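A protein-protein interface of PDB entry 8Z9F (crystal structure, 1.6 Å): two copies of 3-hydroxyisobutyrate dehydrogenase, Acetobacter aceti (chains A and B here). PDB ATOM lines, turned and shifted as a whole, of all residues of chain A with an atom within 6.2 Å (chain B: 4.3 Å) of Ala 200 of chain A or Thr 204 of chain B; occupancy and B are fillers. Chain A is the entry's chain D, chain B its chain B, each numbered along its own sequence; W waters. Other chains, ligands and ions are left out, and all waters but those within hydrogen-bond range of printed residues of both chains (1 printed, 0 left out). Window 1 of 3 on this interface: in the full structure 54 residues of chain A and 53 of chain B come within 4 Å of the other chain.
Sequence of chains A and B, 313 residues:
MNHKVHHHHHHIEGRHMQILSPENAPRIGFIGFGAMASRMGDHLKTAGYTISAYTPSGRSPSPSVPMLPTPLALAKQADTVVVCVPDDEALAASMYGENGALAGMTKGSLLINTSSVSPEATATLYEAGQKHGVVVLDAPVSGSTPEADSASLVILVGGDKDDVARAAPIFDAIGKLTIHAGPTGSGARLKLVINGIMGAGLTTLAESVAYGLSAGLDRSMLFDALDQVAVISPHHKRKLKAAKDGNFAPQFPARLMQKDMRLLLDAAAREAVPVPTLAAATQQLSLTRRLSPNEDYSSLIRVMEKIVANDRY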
ATOM      1  N   ASN A 195      29.718 -16.689   7.242  1.00  0.00           N
ATOM      2  CA  ASN A 195      28.467 -17.448   7.298  1.00  0.00           C
ATOM      3  C   ASN A 195      27.355 -16.764   6.514  1.00  0.00           C
ATOM      4  O   ASN A 195      26.554 -17.436   5.849  1.00  0.00           O
ATOM      5  CB  ASN A 195      28.013 -17.631   8.744  1.00  0.00           C
ATOM      6  CG  ASN A 195      28.695 -18.785   9.415  1.00  0.00           C
ATOM      7  OD1 ASN A 195      28.905 -19.838   8.801  1.00  0.00           O
ATOM      8  ND2 ASN A 195      28.939 -18.648  10.714  1.00  0.00           N
ATOM      9  N   GLY A 196      27.245 -15.439   6.638  1.00  0.00           N
ATOM     10  CA  GLY A 196      26.216 -14.719   5.903  1.00  0.00           C
ATOM     11  C   GLY A 196      26.396 -14.855   4.405  1.00  0.00           C
ATOM     12  O   GLY A 196      25.428 -15.068   3.667  1.00  0.00           O
ATOM     13  N   ILE A 197      27.640 -14.743   3.939  1.00  0.00           N
ATOM     14  CA  ILE A 197      27.925 -14.933   2.520  1.00  0.00           C
ATOM     15  C   ILE A 197      27.524 -16.333   2.082  1.00  0.00           C
ATOM     16  O   ILE A 197      26.902 -16.513   1.026  1.00  0.00           O
ATOM     17  CB  ILE A 197      29.415 -14.648   2.228  1.00  0.00           C
ATOM     18  CG1 ILE A 197      29.739 -13.181   2.511  1.00  0.00           C
ATOM     19  CG2 ILE A 197      29.781 -15.022   0.781  1.00  0.00           C
ATOM     20  CD1 ILE A 197      31.236 -12.906   2.574  1.00  0.00           C
ATOM     21  N   MET A 198      27.853 -17.348   2.895  1.00  0.00           N
ATOM     22  CA  MET A 198      27.545 -18.715   2.512  1.00  0.00           C
ATOM     23  C   MET A 198      26.046 -18.965   2.522  1.00  0.00           C
ATOM     24  O   MET A 198      25.500 -19.527   1.561  1.00  0.00           O
ATOM     25  CB  MET A 198      28.289 -19.691   3.418  1.00  0.00           C
ATOM     26  CG  MET A 198      27.985 -21.135   3.091  1.00  0.00           C
ATOM     27  SD  MET A 198      28.959 -22.148   4.218  1.00  0.00           S
ATOM     28  CE  MET A 198      27.766 -22.165   5.476  1.00  0.00           C
ATOM     29  N   GLY A 199      25.348 -18.501   3.565  1.00  0.00           N
ATOM     30  CA  GLY A 199      23.913 -18.751   3.646  1.00  0.00           C
ATOM     31  C   GLY A 199      23.126 -18.056   2.552  1.00  0.00           C
ATOM     32  O   GLY A 199      22.260 -18.669   1.908  1.00  0.00           O
ATOM     33  N   ALA A 200      23.383 -16.761   2.344  1.00  0.00           N
ATOM     34  CA  ALA A 200      22.671 -16.028   1.300  1.00  0.00           C
ATOM     35  C   ALA A 200      23.117 -16.455  -0.097  1.00  0.00           C
ATOM     36  O   ALA A 200      22.334 -16.374  -1.048  1.00  0.00           O
ATOM     37  CB  ALA A 200      22.858 -14.513   1.502  1.00  0.00           C
ATOM     38  N   GLY A 201      24.345 -16.948  -0.253  1.00  0.00           N
ATOM     39  CA  GLY A 201      24.725 -17.483  -1.551  1.00  0.00           C
ATOM     40  C   GLY A 201      23.875 -18.676  -1.935  1.00  0.00           C
ATOM     41  O   GLY A 201      23.508 -18.853  -3.104  1.00  0.00           O
ATOM     42  N   LEU A 202      23.539 -19.507  -0.955  1.00  0.00           N
ATOM     43  CA  LEU A 202      22.717 -20.672  -1.250  1.00  0.00           C
ATOM     44  C   LEU A 202      21.267 -20.286  -1.508  1.00  0.00           C
ATOM     45  O   LEU A 202      20.648 -20.802  -2.453  1.00  0.00           O
ATOM     46  CB  LEU A 202      22.831 -21.676  -0.103  1.00  0.00           C
ATOM     47  CG  LEU A 202      22.256 -23.088  -0.300  1.00  0.00           C
ATOM     48  CD1 LEU A 202      20.778 -23.139  -0.034  1.00  0.00           C
ATOM     49  CD2 LEU A 202      22.579 -23.670  -1.681  1.00  0.00           C
ATOM     50  N   THR A 203      20.687 -19.392  -0.681  1.00  0.00           N
ATOM     51  CA  THR A 203      19.289 -19.039  -0.916  1.00  0.00           C
ATOM     52  C   THR A 203      19.135 -18.327  -2.256  1.00  0.00           C
ATOM     53  O   THR A 203      18.159 -18.560  -2.981  1.00  0.00           O
ATOM     54  CB  THR A 203      18.703 -18.206   0.247  1.00  0.00           C
ATOM     55  OG1 THR A 203      19.285 -16.890   0.299  1.00  0.00           O
ATOM     56  CG2 THR A 203      18.929 -18.888   1.572  1.00  0.00           C
ATOM     57  N   THR A 204      20.113 -17.488  -2.618  1.00  0.00           N
ATOM     58  CA  THR A 204      20.114 -16.841  -3.930  1.00  0.00           C
ATOM     59  C   THR A 204      20.077 -17.877  -5.045  1.00  0.00           C
ATOM     60  O   THR A 204      19.296 -17.763  -6.002  1.00  0.00           O
ATOM     61  CB  THR A 204      21.363 -15.965  -4.056  1.00  0.00           C
ATOM     62  OG1 THR A 204      21.244 -14.867  -3.145  1.00  0.00           O
ATOM     63  CG2 THR A 204      21.552 -15.439  -5.511  1.00  0.00           C
ATOM     64  N   LEU A 205      20.946 -18.876  -4.942  1.00  0.00           N
ATOM     65  CA  LEU A 205      21.043 -19.906  -5.966  1.00  0.00           C
ATOM     66  C   LEU A 205      19.752 -20.716  -6.049  1.00  0.00           C
ATOM     67  O   LEU A 205      19.232 -20.974  -7.148  1.00  0.00           O
ATOM     68  CB  LEU A 205      22.247 -20.799  -5.659  1.00  0.00           C
ATOM     69  CG  LEU A 205      22.523 -21.924  -6.650  1.00  0.00           C
ATOM     70  CD1 LEU A 205      22.696 -21.350  -8.062  1.00  0.00           C
ATOM     71  CD2 LEU A 205      23.749 -22.720  -6.187  1.00  0.00           C
ATOM     72  N   HIS A 236      29.501 -23.139  -3.683  1.00  0.00           N
ATOM     73  CA  HIS A 236      28.111 -23.304  -4.084  1.00  0.00           C
ATOM     74  C   HIS A 236      27.980 -24.109  -5.374  1.00  0.00           C
ATOM     75  O   HIS A 236      26.961 -24.772  -5.579  1.00  0.00           O
ATOM     76  CB  HIS A 236      27.437 -21.931  -4.195  1.00  0.00           C
ATOM     77  CG  HIS A 236      27.267 -21.241  -2.869  1.00  0.00           C
ATOM     78  ND1 HIS A 236      28.060 -20.180  -2.471  1.00  0.00           N
ATOM     79  CD2 HIS A 236      26.408 -21.467  -1.846  1.00  0.00           C
ATOM     80  CE1 HIS A 236      27.684 -19.773  -1.270  1.00  0.00           C
ATOM     81  NE2 HIS A 236      26.693 -20.546  -0.862  1.00  0.00           N
ATOM     82  N   MET A 261      22.800 -18.091  10.952  1.00  0.00           N
ATOM     83  CA  MET A 261      22.093 -16.954  10.373  1.00  0.00           C
ATOM     84  C   MET A 261      21.380 -16.154  11.460  1.00  0.00           C
ATOM     85  O   MET A 261      21.385 -14.920  11.445  1.00  0.00           O
ATOM     86  CB  MET A 261      21.098 -17.491   9.349  1.00  0.00           C
ATOM     87  CG  MET A 261      21.623 -17.853   7.935  1.00  0.00           C
ATOM     88  SD  MET A 261      23.014 -16.973   7.200  1.00  0.00           S
ATOM     89  CE  MET A 261      22.053 -15.727   6.326  1.00  0.00           C
ATOM     90  N   THR A 277      19.283  -8.386   2.436  1.00  0.00           N
ATOM     91  CA  THR A 277      19.504  -9.645   1.716  1.00  0.00           C
ATOM     92  C   THR A 277      19.773 -10.778   2.697  1.00  0.00           C
ATOM     93  O   THR A 277      19.224 -11.879   2.566  1.00  0.00           O
ATOM     94  CB  THR A 277      20.664  -9.535   0.716  1.00  0.00           C
ATOM     95  OG1 THR A 277      20.528  -8.358  -0.090  1.00  0.00           O
ATOM     96  CG2 THR A 277      20.673 -10.758  -0.225  1.00  0.00           C
ATOM     97  N   LEU A 278      20.596 -10.511   3.715  1.00  0.00           N
ATOM     98  CA  LEU A 278      20.894 -11.538   4.712  1.00  0.00           C
ATOM     99  C   LEU A 278      19.657 -11.883   5.527  1.00  0.00           C
ATOM    100  O   LEU A 278      19.466 -13.045   5.908  1.00  0.00           O
ATOM    101  CB  LEU A 278      22.023 -11.067   5.631  1.00  0.00           C
ATOM    102  CG  LEU A 278      23.314 -10.650   4.937  1.00  0.00           C
ATOM    103  CD1 LEU A 278      24.310 -10.149   5.977  1.00  0.00           C
ATOM    104  CD2 LEU A 278      23.889 -11.793   4.105  1.00  0.00           C
ATOM    105  N   ALA A 281      17.468 -14.155   3.394  1.00  0.00           N
ATOM    106  CA  ALA A 281      18.090 -15.476   3.348  1.00  0.00           C
ATOM    107  C   ALA A 281      17.824 -16.260   4.626  1.00  0.00           C
ATOM    108  O   ALA A 281      17.561 -17.469   4.575  1.00  0.00           O
ATOM    109  CB  ALA A 281      19.587 -15.328   3.126  1.00  0.00           C
ATOM    110  N   LEU A 285      16.185 -20.014   5.239  1.00  0.00           N
ATOM    111  CA  LEU A 285      16.860 -21.079   5.952  1.00  0.00           C
ATOM    112  C   LEU A 285      16.088 -21.526   7.190  1.00  0.00           C
ATOM    113  O   LEU A 285      16.222 -22.687   7.606  1.00  0.00           O
ATOM    114  CB  LEU A 285      18.285 -20.634   6.284  1.00  0.00           C
ATOM    115  CG  LEU A 285      19.100 -20.588   4.989  1.00  0.00           C
ATOM    116  CD1 LEU A 285      20.344 -19.744   5.154  1.00  0.00           C
ATOM    117  CD2 LEU A 285      19.433 -22.020   4.544  1.00  0.00           C
ATOM    118  N   ALA B 200      22.337 -10.506  -6.453  1.00  0.00           N
ATOM    119  CA  ALA B 200      22.226 -10.836  -5.043  1.00  0.00           C
ATOM    120  C   ALA B 200      23.566 -11.264  -4.470  1.00  0.00           C
ATOM    121  O   ALA B 200      23.791 -11.110  -3.272  1.00  0.00           O
ATOM    122  CB  ALA B 200      21.177 -11.933  -4.821  1.00  0.00           C
ATOM    123  N   GLY B 201      24.458 -11.833  -5.290  1.00  0.00           N
ATOM    124  CA  GLY B 201      25.806 -12.102  -4.806  1.00  0.00           C
ATOM    125  C   GLY B 201      26.497 -10.832  -4.343  1.00  0.00           C
ATOM    126  O   GLY B 201      27.167 -10.813  -3.304  1.00  0.00           O
ATOM    127  N   LEU B 202      26.298  -9.734  -5.085  1.00  0.00           N
ATOM    128  CA  LEU B 202      26.919  -8.472  -4.711  1.00  0.00           C
ATOM    129  C   LEU B 202      26.258  -7.882  -3.467  1.00  0.00           C
ATOM    130  O   LEU B 202      26.949  -7.405  -2.560  1.00  0.00           O
ATOM    131  CB  LEU B 202      26.850  -7.490  -5.883  1.00  0.00           C
ATOM    132  CG  LEU B 202      27.662  -6.185  -5.753  1.00  0.00           C
ATOM    133  CD1 LEU B 202      26.923  -5.111  -4.902  1.00  0.00           C
ATOM    134  CD2 LEU B 202      29.053  -6.471  -5.198  1.00  0.00           C
ATOM    135  N   THR B 203      24.918  -7.883  -3.404  1.00  0.00           N
ATOM    136  CA  THR B 203      24.289  -7.268  -2.232  1.00  0.00           C
ATOM    137  C   THR B 203      24.610  -8.060  -0.968  1.00  0.00           C
ATOM    138  O   THR B 203      24.834  -7.463   0.100  1.00  0.00           O
ATOM    139  CB  THR B 203      22.773  -7.114  -2.412  1.00  0.00           C
ATOM    140  OG1 THR B 203      22.141  -8.398  -2.466  1.00  0.00           O
ATOM    141  CG2 THR B 203      22.451  -6.317  -3.683  1.00  0.00           C
ATOM    142  N   THR B 204      24.651  -9.390  -1.080  1.00  0.00           N
ATOM    143  CA  THR B 204      25.063 -10.234   0.035  1.00  0.00           C
ATOM    144  C   THR B 204      26.451  -9.845   0.511  1.00  0.00           C
ATOM    145  O   THR B 204      26.694  -9.692   1.710  1.00  0.00           O
ATOM    146  CB  THR B 204      25.056 -11.698  -0.403  1.00  0.00           C
ATOM    147  OG1 THR B 204      23.706 -12.127  -0.618  1.00  0.00           O
ATOM    148  CG2 THR B 204      25.738 -12.602   0.639  1.00  0.00           C
ATOM    149  N   LEU B 205      27.385  -9.708  -0.432  1.00  0.00           N
ATOM    150  CA  LEU B 205      28.756  -9.371  -0.064  1.00  0.00           C
ATOM    151  C   LEU B 205      28.832  -7.988   0.569  1.00  0.00           C
ATOM    152  O   LEU B 205      29.525  -7.799   1.579  1.00  0.00           O
ATOM    153  CB  LEU B 205      29.654  -9.459  -1.298  1.00  0.00           C
ATOM    154  CG  LEU B 205      31.133  -9.137  -1.093  1.00  0.00           C
ATOM    155  CD1 LEU B 205      31.774 -10.064  -0.076  1.00  0.00           C
ATOM    156  CD2 LEU B 205      31.851  -9.245  -2.428  1.00  0.00           C
ATOM    157  N   ALA B 206      28.101  -7.010   0.019  1.00  0.00           N
ATOM    158  CA  ALA B 206      28.166  -5.661   0.575  1.00  0.00           C
ATOM    159  C   ALA B 206      27.644  -5.622   2.004  1.00  0.00           C
ATOM    160  O   ALA B 206      28.221  -4.946   2.869  1.00  0.00           O
ATOM    161  CB  ALA B 206      27.377  -4.702  -0.310  1.00  0.00           C
ATOM    162  N   GLU B 207      26.538  -6.327   2.261  1.00  0.00           N
ATOM    163  CA  GLU B 207      25.930  -6.339   3.588  1.00  0.00           C
ATOM    164  C   GLU B 207      26.819  -7.036   4.585  1.00  0.00           C
ATOM    165  O   GLU B 207      26.930  -6.585   5.725  1.00  0.00           O
ATOM    166  CB  GLU B 207      24.560  -7.011   3.531  1.00  0.00           C
ATOM    167  CG  GLU B 207      23.633  -6.249   2.633  1.00  0.00           C
ATOM    168  CD  GLU B 207      22.312  -6.938   2.461  1.00  0.00           C
ATOM    169  OE1 GLU B 207      21.524  -6.477   1.612  1.00  0.00           O
ATOM    170  OE2 GLU B 207      22.037  -7.893   3.210  1.00  0.00           O
ATOM    171  N   SER B 208      27.451  -8.136   4.167  1.00  0.00           N
ATOM    172  CA  SER B 208      28.315  -8.910   5.056  1.00  0.00           C
ATOM    173  C   SER B 208      29.569  -8.131   5.416  1.00  0.00           C
ATOM    174  O   SER B 208      29.946  -8.080   6.596  1.00  0.00           O
ATOM    175  CB  SER B 208      28.660 -10.245   4.401  1.00  0.00           C
ATOM    176  OG  SER B 208      27.469 -11.004   4.168  1.00  0.00           O
HETATM  177  O   HOH W   1      24.467 -14.424  -2.735  1.00  0.00           O
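Of the 9 printed residues of chain B, 6 touch a printed residue of chain A. Hydrophobic or aromatic side chains of chain B within 4 Å of the printed part of chain A: Ala 200 and Leu 205. Along chain B the printed residues that touch a printed residue of chain A span positions 200 to 208. Of the 17 printed residues of chain A, 6 touch a printed residue of chain B. Printed residues of chain A that touch a printed residue of chain B: Gly 196, Ile 197, Ala 200, Thr 204, Thr 277 and Leu 278. Among the printed residues, no Asp or Glu carboxylate lies within 4 Å of a Lys or Arg side-chain nitrogen of the other chain.
The side-chain hydroxyl (OG1) of Thr 203 of chain B is in hydrogen-bond range of the backbone carbonyl oxygen (O) of Ala 200 of chain B, 3.3 Å away. OG1 of Thr 204 of chain B sits at hydrogen-bond distance from O of Ala 200 of chain B (2.8 Å). O of Thr 204 of chain B lies within hydrogen-bond range of OG of Ser 208 of chain B. OG1 of Thr 203 of chain A sits at hydrogen-bond distance from O of Ala 200 of chain A, at 3.4 Å. O of Ala 200 of chain A is in hydrogen-bond range of OG1 of Thr 204 of chain A (2.8 Å).
Ala 200 of chain A touches just one residue of chain B: Thr 204 (3.3 Å). Of the printed residues of chain A, Thr 204 of chain B touches Gly 196, Ile 197, Ala 200 and Thr 277. Of the printed residues of chain B, Gly 196 of chain A touches Thr 204 (3.9 Å). Printed residues of chain A within 4 Å of Ser 208 of chain B: Ile 197 (3.6 Å) and Leu 278 (3.7 Å). The nearest printed residue of chain B that does not touch Ala 200 of chain A is Ala 200 of chain B (5.9 Å). The nearest printed residue of chain A that does not touch Thr 204 of chain B is Leu 278 of chain A (4.01 Å).
OG1 of Thr 277 of chain A is in hydrogen-bond range of OG1 of Thr 203 of chain B. OG1 of Thr 277 of chain A lies within hydrogen-bond range of OE1 of Glu 207 of chain B. The side-chain carboxylate (OE2) of Glu 207 of chain B is in hydrogen-bond range of the backbone NH (N) of Leu 278 of chain A, 3.0 Å away.
Among the printed residues, pairs that only touch across the chains: Gly 196 of chain A with Thr 204 of chain B (3.9 Å), Ile 197 of chain A with Thr 204 of chain B (3.7 Å), Ile 197 of chain A with Leu 205 of chain B (3.9 Å), Ile 197 of chain A with Ser 208 of chain B (3.6 Å), Ala 200 of chain A with Thr 204 of chain B (3.3 Å), Thr 204 of chain A with Ala 200 of chain B (3.4 Å), Thr 277 of chain A with Thr 204 of chain B (3.4 Å) and Leu 278 of chain A with Ser 208 of chain B (3.7 Å).
Water W1 lies within hydrogen-bond range of the side-chain hydroxyl of Thr 204 of chain B (3.2 Å), the side-chain hydroxyl of Thr 204 of chain A (3.3 Å), the backbone carbonyl oxygen of Ala 200 of chain A (3.3 Å) and the backbone carbonyl oxygen of Ala 200 of chain B (3.4 Å).
Ala 200 of chain A touches Thr 204 of chain B, and with the chains exchanged Thr 204 of chain A touches Ala 200 of chain B. Of the 11 pairs that touch across the chains among the printed residues, 2 have their exchanged pair printed and touching as well.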
